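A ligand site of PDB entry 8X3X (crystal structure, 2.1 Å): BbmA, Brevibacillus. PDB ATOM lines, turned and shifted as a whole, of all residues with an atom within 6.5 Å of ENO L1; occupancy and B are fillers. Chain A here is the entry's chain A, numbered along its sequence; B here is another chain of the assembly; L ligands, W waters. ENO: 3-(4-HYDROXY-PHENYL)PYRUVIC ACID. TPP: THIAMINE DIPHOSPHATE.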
ATOM      1  N   TRP A 292       7.387 -19.701  -0.394  1.00  0.00           N
ATOM      2  CA  TRP A 292       6.833 -18.716  -1.323  1.00  0.00           C
ATOM      3  C   TRP A 292       7.587 -17.394  -1.291  1.00  0.00           C
ATOM      4  O   TRP A 292       7.546 -16.656  -2.274  1.00  0.00           O
ATOM      5  CB  TRP A 292       5.351 -18.505  -0.997  1.00  0.00           C
ATOM      6  CG  TRP A 292       4.493 -19.578  -1.624  1.00  0.00           C
ATOM      7  CD1 TRP A 292       4.940 -20.693  -2.306  1.00  0.00           C
ATOM      8  CD2 TRP A 292       3.077 -19.645  -1.643  1.00  0.00           C
ATOM      9  NE1 TRP A 292       3.873 -21.431  -2.742  1.00  0.00           N
ATOM     10  CE2 TRP A 292       2.716 -20.813  -2.343  1.00  0.00           C
ATOM     11  CE3 TRP A 292       2.064 -18.830  -1.137  1.00  0.00           C
ATOM     12  CZ2 TRP A 292       1.393 -21.179  -2.539  1.00  0.00           C
ATOM     13  CZ3 TRP A 292       0.755 -19.191  -1.334  1.00  0.00           C
ATOM     14  CH2 TRP A 292       0.426 -20.363  -2.035  1.00  0.00           C
ATOM     15  N   LEU A 484      -7.686 -24.370  -8.464  1.00  0.00           N
ATOM     16  CA  LEU A 484      -6.281 -24.760  -8.372  1.00  0.00           C
ATOM     17  C   LEU A 484      -6.111 -26.264  -8.488  1.00  0.00           C
ATOM     18  O   LEU A 484      -5.183 -26.742  -9.163  1.00  0.00           O
ATOM     19  CB  LEU A 484      -5.680 -24.243  -7.068  1.00  0.00           C
ATOM     20  CG  LEU A 484      -5.473 -22.723  -6.956  1.00  0.00           C
ATOM     21  CD1 LEU A 484      -4.474 -22.407  -5.823  1.00  0.00           C
ATOM     22  CD2 LEU A 484      -5.014 -22.106  -8.272  1.00  0.00           C
ATOM     23  N   VAL A 485      -6.983 -27.047  -7.848  1.00  0.00           N
ATOM     24  CA  VAL A 485      -6.870 -28.510  -7.943  1.00  0.00           C
ATOM     25  C   VAL A 485      -7.143 -28.965  -9.361  1.00  0.00           C
ATOM     26  O   VAL A 485      -6.437 -29.834  -9.896  1.00  0.00           O
ATOM     27  CB  VAL A 485      -7.824 -29.207  -6.953  1.00  0.00           C
ATOM     28  CG1 VAL A 485      -7.659 -30.743  -7.077  1.00  0.00           C
ATOM     29  CG2 VAL A 485      -7.592 -28.744  -5.533  1.00  0.00           C
ATOM     30  N   HIS A 486      -8.178 -28.407  -9.990  1.00  0.00           N
ATOM     31  CA  HIS A 486      -8.494 -28.704 -11.377  1.00  0.00           C
ATOM     32  C   HIS A 486      -7.291 -28.455 -12.270  1.00  0.00           C
ATOM     33  O   HIS A 486      -6.945 -29.290 -13.117  1.00  0.00           O
ATOM     34  CB  HIS A 486      -9.694 -27.857 -11.815  1.00  0.00           C
ATOM     35  CG  HIS A 486     -10.181 -28.136 -13.202  1.00  0.00           C
ATOM     36  ND1 HIS A 486     -11.068 -29.150 -13.489  1.00  0.00           N
ATOM     37  CD2 HIS A 486      -9.915 -27.511 -14.376  1.00  0.00           C
ATOM     38  CE1 HIS A 486     -11.313 -29.148 -14.790  1.00  0.00           C
ATOM     39  NE2 HIS A 486     -10.630 -28.164 -15.352  1.00  0.00           N
ATOM     40  N   LEU A 487      -6.612 -27.315 -12.080  1.00  0.00           N
ATOM     41  CA  LEU A 487      -5.449 -27.016 -12.894  1.00  0.00           C
ATOM     42  C   LEU A 487      -4.293 -27.967 -12.587  1.00  0.00           C
ATOM     43  O   LEU A 487      -3.544 -28.346 -13.499  1.00  0.00           O
ATOM     44  CB  LEU A 487      -5.017 -25.564 -12.690  1.00  0.00           C
ATOM     45  CG  LEU A 487      -5.964 -24.493 -13.230  1.00  0.00           C
ATOM     46  CD1 LEU A 487      -5.700 -23.134 -12.547  1.00  0.00           C
ATOM     47  CD2 LEU A 487      -5.852 -24.388 -14.760  1.00  0.00           C
ATOM     48  N   GLY A 488      -4.147 -28.372 -11.332  1.00  0.00           N
ATOM     49  CA  GLY A 488      -3.150 -29.375 -10.991  1.00  0.00           C
ATOM     50  C   GLY A 488      -3.421 -30.727 -11.643  1.00  0.00           C
ATOM     51  O   GLY A 488      -2.489 -31.416 -12.063  1.00  0.00           O
ATOM     52  N   GLU A 489      -4.693 -31.130 -11.739  1.00  0.00           N
ATOM     53  CA  GLU A 489      -5.014 -32.353 -12.457  1.00  0.00           C
ATOM     54  C   GLU A 489      -4.560 -32.284 -13.906  1.00  0.00           C
ATOM     55  O   GLU A 489      -3.988 -33.243 -14.436  1.00  0.00           O
ATOM     56  CB  GLU A 489      -6.524 -32.636 -12.406  1.00  0.00           C
ATOM     57  CG  GLU A 489      -7.079 -32.930 -11.017  1.00  0.00           C
ATOM     58  CD  GLU A 489      -8.553 -32.600 -10.920  1.00  0.00           C
ATOM     59  OE1 GLU A 489      -9.121 -32.770  -9.819  1.00  0.00           O
ATOM     60  OE2 GLU A 489      -9.150 -32.173 -11.938  1.00  0.00           O
ATOM     61  N   GLN A 492      -0.329 -31.691 -13.842  1.00  0.00           N
ATOM     62  CA  GLN A 492       0.506 -32.635 -13.134  1.00  0.00           C
ATOM     63  C   GLN A 492       0.044 -34.086 -13.246  1.00  0.00           C
ATOM     64  O   GLN A 492       0.868 -34.983 -13.032  1.00  0.00           O
ATOM     65  CB  GLN A 492       0.560 -32.288 -11.635  1.00  0.00           C
ATOM     66  CG  GLN A 492       1.340 -31.067 -11.255  1.00  0.00           C
ATOM     67  CD  GLN A 492       1.323 -30.888  -9.760  1.00  0.00           C
ATOM     68  OE1 GLN A 492       0.377 -30.324  -9.210  1.00  0.00           O
ATOM     69  NE2 GLN A 492       2.321 -31.433  -9.080  1.00  0.00           N
ATOM     70  N   PHE A 493      -1.226 -34.340 -13.522  1.00  0.00           N
ATOM     71  CA  PHE A 493      -1.744 -35.703 -13.587  1.00  0.00           C
ATOM     72  C   PHE A 493      -2.455 -35.966 -14.911  1.00  0.00           C
ATOM     73  O   PHE A 493      -3.338 -36.827 -14.988  1.00  0.00           O
ATOM     74  CB  PHE A 493      -2.659 -35.973 -12.388  1.00  0.00           C
ATOM     75  CG  PHE A 493      -1.938 -35.959 -11.056  1.00  0.00           C
ATOM     76  CD1 PHE A 493      -1.805 -34.778 -10.333  1.00  0.00           C
ATOM     77  CD2 PHE A 493      -1.381 -37.120 -10.537  1.00  0.00           C
ATOM     78  CE1 PHE A 493      -1.126 -34.756  -9.121  1.00  0.00           C
ATOM     79  CE2 PHE A 493      -0.711 -37.115  -9.323  1.00  0.00           C
ATOM     80  CZ  PHE A 493      -0.584 -35.922  -8.610  1.00  0.00           C
ATOM     81  N   MET A 557       1.152 -19.536 -11.607  1.00  0.00           N
ATOM     82  CA  MET A 557       0.850 -20.888 -11.284  1.00  0.00           C
ATOM     83  C   MET A 557       1.629 -21.746 -12.245  1.00  0.00           C
ATOM     84  O   MET A 557       2.252 -22.719 -11.863  1.00  0.00           O
ATOM     85  CB  MET A 557      -0.622 -21.152 -11.417  1.00  0.00           C
ATOM     86  CG  MET A 557      -1.125 -22.199 -10.490  1.00  0.00           C
ATOM     87  SD  MET A 557      -1.049 -21.775  -8.767  1.00  0.00           S
ATOM     88  CE  MET A 557      -1.153 -23.400  -8.084  1.00  0.00           C
ATOM     89  N   ARG A 560       4.883 -22.505 -11.244  1.00  0.00           N
ATOM     90  CA  ARG A 560       4.755 -23.432 -10.178  1.00  0.00           C
ATOM     91  C   ARG A 560       4.222 -24.730 -10.788  1.00  0.00           C
ATOM     92  O   ARG A 560       4.153 -24.895 -11.997  1.00  0.00           O
ATOM     93  CB  ARG A 560       3.771 -22.926  -9.159  1.00  0.00           C
ATOM     94  CG  ARG A 560       4.035 -23.282  -7.724  1.00  0.00           C
ATOM     95  CD  ARG A 560       2.751 -23.749  -7.061  1.00  0.00           C
ATOM     96  NE  ARG A 560       3.021 -24.464  -5.833  1.00  0.00           N
ATOM     97  CZ  ARG A 560       2.094 -25.006  -5.066  1.00  0.00           C
ATOM     98  NH1 ARG A 560       0.836 -24.892  -5.409  1.00  0.00           N
ATOM     99  NH2 ARG A 560       2.432 -25.645  -3.977  1.00  0.00           N
ATOM    100  N   PHE A 561       3.941 -25.686  -9.871  1.00  0.00           N
ATOM    101  CA  PHE A 561       3.498 -27.122  -9.964  1.00  0.00           C
ATOM    102  C   PHE A 561       4.732 -28.048 -10.155  1.00  0.00           C
ATOM    103  O   PHE A 561       4.638 -29.260 -10.095  1.00  0.00           O
ATOM    104  CB  PHE A 561       2.625 -27.562 -11.166  1.00  0.00           C
ATOM    105  CG  PHE A 561       1.262 -26.928 -11.288  1.00  0.00           C
ATOM    106  CD1 PHE A 561       0.277 -27.185 -10.407  1.00  0.00           C
ATOM    107  CD2 PHE A 561       0.940 -26.209 -12.394  1.00  0.00           C
ATOM    108  CE1 PHE A 561      -0.967 -26.669 -10.569  1.00  0.00           C
ATOM    109  CE2 PHE A 561      -0.305 -25.695 -12.575  1.00  0.00           C
ATOM    110  CZ  PHE A 561      -1.265 -25.926 -11.657  1.00  0.00           C
ATOM    111  N   PRO B  29      -9.158 -32.607  -1.513  1.00  0.00           N
ATOM    112  CA  PRO B  29      -7.774 -32.740  -1.979  1.00  0.00           C
ATOM    113  C   PRO B  29      -6.916 -31.538  -1.623  1.00  0.00           C
ATOM    114  O   PRO B  29      -7.387 -30.480  -1.187  1.00  0.00           O
ATOM    115  CB  PRO B  29      -7.925 -32.874  -3.507  1.00  0.00           C
ATOM    116  CG  PRO B  29      -9.191 -32.102  -3.786  1.00  0.00           C
ATOM    117  CD  PRO B  29     -10.105 -32.455  -2.631  1.00  0.00           C
ATOM    118  N   GLY B  30      -5.613 -31.737  -1.809  1.00  0.00           N
ATOM    119  CA  GLY B  30      -4.603 -30.689  -1.702  1.00  0.00           C
ATOM    120  C   GLY B  30      -3.368 -31.177  -2.426  1.00  0.00           C
ATOM    121  O   GLY B  30      -3.197 -32.379  -2.644  1.00  0.00           O
ATOM    122  N   GLY B  31      -2.509 -30.229  -2.815  1.00  0.00           N
ATOM    123  CA  GLY B  31      -1.321 -30.540  -3.569  1.00  0.00           C
ATOM    124  C   GLY B  31      -0.582 -31.780  -3.065  1.00  0.00           C
ATOM    125  O   GLY B  31      -0.403 -32.758  -3.801  1.00  0.00           O
ATOM    126  N   PRO B  32      -0.156 -31.752  -1.807  1.00  0.00           N
ATOM    127  CA  PRO B  32       0.627 -32.886  -1.253  1.00  0.00           C
ATOM    128  C   PRO B  32      -0.188 -34.161  -1.115  1.00  0.00           C
ATOM    129  O   PRO B  32       0.407 -35.245  -0.975  1.00  0.00           O
ATOM    130  CB  PRO B  32       1.084 -32.370   0.119  1.00  0.00           C
ATOM    131  CG  PRO B  32       0.826 -30.880   0.111  1.00  0.00           C
ATOM    132  CD  PRO B  32      -0.282 -30.634  -0.853  1.00  0.00           C
ATOM    133  N   MET B  34      -2.351 -35.185  -3.523  1.00  0.00           N
ATOM    134  CA  MET B  34      -2.801 -35.643  -4.830  1.00  0.00           C
ATOM    135  C   MET B  34      -2.359 -37.057  -5.180  1.00  0.00           C
ATOM    136  O   MET B  34      -3.107 -37.745  -5.890  1.00  0.00           O
ATOM    137  CB  MET B  34      -2.343 -34.656  -5.921  1.00  0.00           C
ATOM    138  CG  MET B  34      -3.056 -33.302  -5.831  1.00  0.00           C
ATOM    139  SD  MET B  34      -4.855 -33.416  -5.955  1.00  0.00           S
ATOM    140  CE  MET B  34      -5.044 -33.524  -7.744  1.00  0.00           C
ATOM    141  N   THR B  77      -5.424 -32.469   3.453  1.00  0.00           N
ATOM    142  CA  THR B  77      -4.115 -31.987   3.059  1.00  0.00           C
ATOM    143  C   THR B  77      -3.335 -31.488   4.272  1.00  0.00           C
ATOM    144  O   THR B  77      -3.780 -31.570   5.420  1.00  0.00           O
ATOM    145  CB  THR B  77      -4.233 -30.882   2.005  1.00  0.00           C
ATOM    146  OG1 THR B  77      -2.949 -30.666   1.410  1.00  0.00           O
ATOM    147  CG2 THR B  77      -4.761 -29.566   2.628  1.00  0.00           C
ATOM    148  N   THR B  78      -2.135 -30.985   4.014  1.00  0.00           N
ATOM    149  CA  THR B  78      -1.289 -30.434   5.069  1.00  0.00           C
ATOM    150  C   THR B  78      -2.018 -29.329   5.829  1.00  0.00           C
ATOM    151  O   THR B  78      -3.020 -28.783   5.370  1.00  0.00           O
ATOM    152  CB  THR B  78       0.007 -29.878   4.459  1.00  0.00           C
ATOM    153  OG1 THR B  78      -0.310 -29.255   3.200  1.00  0.00           O
ATOM    154  CG2 THR B  78       0.985 -31.001   4.177  1.00  0.00           C
ATOM    155  N   LEU B 116       5.459 -24.719   2.604  1.00  0.00           N
ATOM    156  CA  LEU B 116       4.053 -24.330   2.501  1.00  0.00           C
ATOM    157  C   LEU B 116       3.213 -25.264   3.360  1.00  0.00           C
ATOM    158  O   LEU B 116       3.258 -26.476   3.201  1.00  0.00           O
ATOM    159  CB  LEU B 116       3.605 -24.391   1.036  1.00  0.00           C
ATOM    160  CG  LEU B 116       2.099 -24.222   0.804  1.00  0.00           C
ATOM    161  CD1 LEU B 116       1.641 -22.845   1.268  1.00  0.00           C
ATOM    162  CD2 LEU B 116       1.720 -24.461  -0.652  1.00  0.00           C
ATOM    163  N   GLN B 117       2.475 -24.685   4.309  1.00  0.00           N
ATOM    164  CA  GLN B 117       1.653 -25.452   5.236  1.00  0.00           C
ATOM    165  C   GLN B 117       2.467 -26.530   5.954  1.00  0.00           C
ATOM    166  O   GLN B 117       1.959 -27.600   6.291  1.00  0.00           O
ATOM    167  CB  GLN B 117       0.442 -26.059   4.518  1.00  0.00           C
ATOM    168  CG  GLN B 117      -0.492 -24.981   3.896  1.00  0.00           C
ATOM    169  CD  GLN B 117      -1.662 -25.569   3.115  1.00  0.00           C
ATOM    170  OE1 GLN B 117      -1.595 -26.699   2.657  1.00  0.00           O
ATOM    171  NE2 GLN B 117      -2.741 -24.787   2.965  1.00  0.00           N
HETATM  172  O4  ENO L   1      -3.726 -27.316  -2.362  1.00  0.00           O
HETATM  173  C9  ENO L   1      -2.118 -27.398  -6.270  1.00  0.00           C
HETATM  174  C8  ENO L   1      -1.716 -28.439  -7.106  1.00  0.00           C
HETATM  175  C7  ENO L   1      -2.430 -29.635  -7.140  1.00  0.00           C
HETATM  176  C6  ENO L   1      -3.559 -29.796  -6.347  1.00  0.00           C
HETATM  177  C5  ENO L   1      -3.971 -28.753  -5.531  1.00  0.00           C
HETATM  178  C4  ENO L   1      -3.262 -27.565  -5.497  1.00  0.00           C
HETATM  179  O3  ENO L   1      -2.024 -30.690  -7.975  1.00  0.00           O
HETATM  180  C3  ENO L   1      -3.729 -26.459  -4.551  1.00  0.00           C
HETATM  181  C2  ENO L   1      -3.099 -26.768  -3.202  1.00  0.00           C
HETATM  182  C1  ENO L   1      -1.635 -26.413  -2.974  1.00  0.00           C
HETATM  183  O2  ENO L   1      -0.927 -27.121  -2.224  1.00  0.00           O
HETATM  184  O1  ENO L   1      -1.124 -25.413  -3.557  1.00  0.00           O
HETATM  185  N1' TPP L   2      -8.449 -27.414   2.701  1.00  0.00           N
HETATM  186  C2' TPP L   2      -8.191 -26.247   3.337  1.00  0.00           C
HETATM  187  CM2 TPP L   2      -8.944 -25.986   4.600  1.00  0.00           C
HETATM  188  N3' TPP L   2      -7.328 -25.312   2.938  1.00  0.00           N
HETATM  189  C4' TPP L   2      -6.653 -25.533   1.798  1.00  0.00           C
HETATM  190  N4' TPP L   2      -5.775 -24.593   1.418  1.00  0.00           N
HETATM  191  C5' TPP L   2      -6.841 -26.734   1.050  1.00  0.00           C
HETATM  192  C6' TPP L   2      -7.764 -27.616   1.569  1.00  0.00           C
HETATM  193  C7' TPP L   2      -6.116 -27.027  -0.229  1.00  0.00           C
HETATM  194  N3  TPP L   2      -6.509 -26.116  -1.324  1.00  0.00           N
HETATM  195  C2  TPP L   2      -5.789 -25.088  -1.720  1.00  0.00           C
HETATM  196  S1  TPP L   2      -6.527 -24.234  -2.960  1.00  0.00           S
HETATM  197  C5  TPP L   2      -7.874 -25.316  -2.944  1.00  0.00           C
HETATM  198  C4  TPP L   2      -7.732 -26.253  -1.993  1.00  0.00           C
HETATM  199  CM4 TPP L   2      -8.675 -27.346  -1.659  1.00  0.00           C
HETATM  200  C6  TPP L   2      -9.050 -25.052  -3.835  1.00  0.00           C
HETATM  201  C7  TPP L   2      -9.707 -23.733  -3.485  1.00  0.00           C
HETATM  202  O7  TPP L   2     -10.928 -23.568  -4.246  1.00  0.00           O
HETATM  203  PA  TPP L   2     -11.733 -22.214  -4.282  1.00  0.00           P
HETATM  204  O1A TPP L   2     -11.889 -21.559  -2.963  1.00  0.00           O
HETATM  205  O2A TPP L   2     -13.051 -22.426  -5.041  1.00  0.00           O
HETATM  206  O3A TPP L   2     -10.777 -21.379  -5.222  1.00  0.00           O
HETATM  207  PB  TPP L   2     -10.287 -21.368  -6.739  1.00  0.00           P
HETATM  208  O1B TPP L   2     -10.230 -19.960  -7.252  1.00  0.00           O
HETATM  209  O2B TPP L   2     -11.312 -22.278  -7.457  1.00  0.00           O
HETATM  210  O3B TPP L   2      -8.948 -22.114  -6.738  1.00  0.00           O
HETATM  211  O   HOH W   1      -2.519 -28.167   0.546  1.00  0.00           O
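An oxygen (O3) of ENO L1 sits at hydrogen-bond distance from the side-chain amide oxygen of Gln 492.
The guanidinium group (NH1) of Arg 560 lies within salt-bridge range of an oxygen (O1) of ENO L1 (2.7 Å).
The backbone NH of Gly 31 of chain B sits at hydrogen-bond distance from an oxygen (O4) of ENO L1, 3.2 Å away.
The backbone NH (N) of Leu 484 lies within hydrogen-bond range of an oxygen (O3B) of TPP L2 (3.1 Å).
N4' of TPP L2 lies close to NE2 of Gln 117 of chain B, at 3.4 Å.
O of Phe 561 lies within hydrogen-bond range of NE2 of Gln 492 (3.3 Å).
Merely in contact with ENO L1: Gly 488, Met 34 of chain B, Gly 30 of chain B, Val 485, Pro 32 of chain B, Leu 484 and Phe 561.
Hydrophobic or aromatic side chains within 4 Å of ENO L1: Leu 484, Val 485, Phe 561, Pro 32 of chain B and Met 34 of chain B.
Water W1 lies within hydrogen-bond range of OG1 of Thr 77 of chain B, OE1 of Gln 117 of chain B and O4 of ENO L1.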
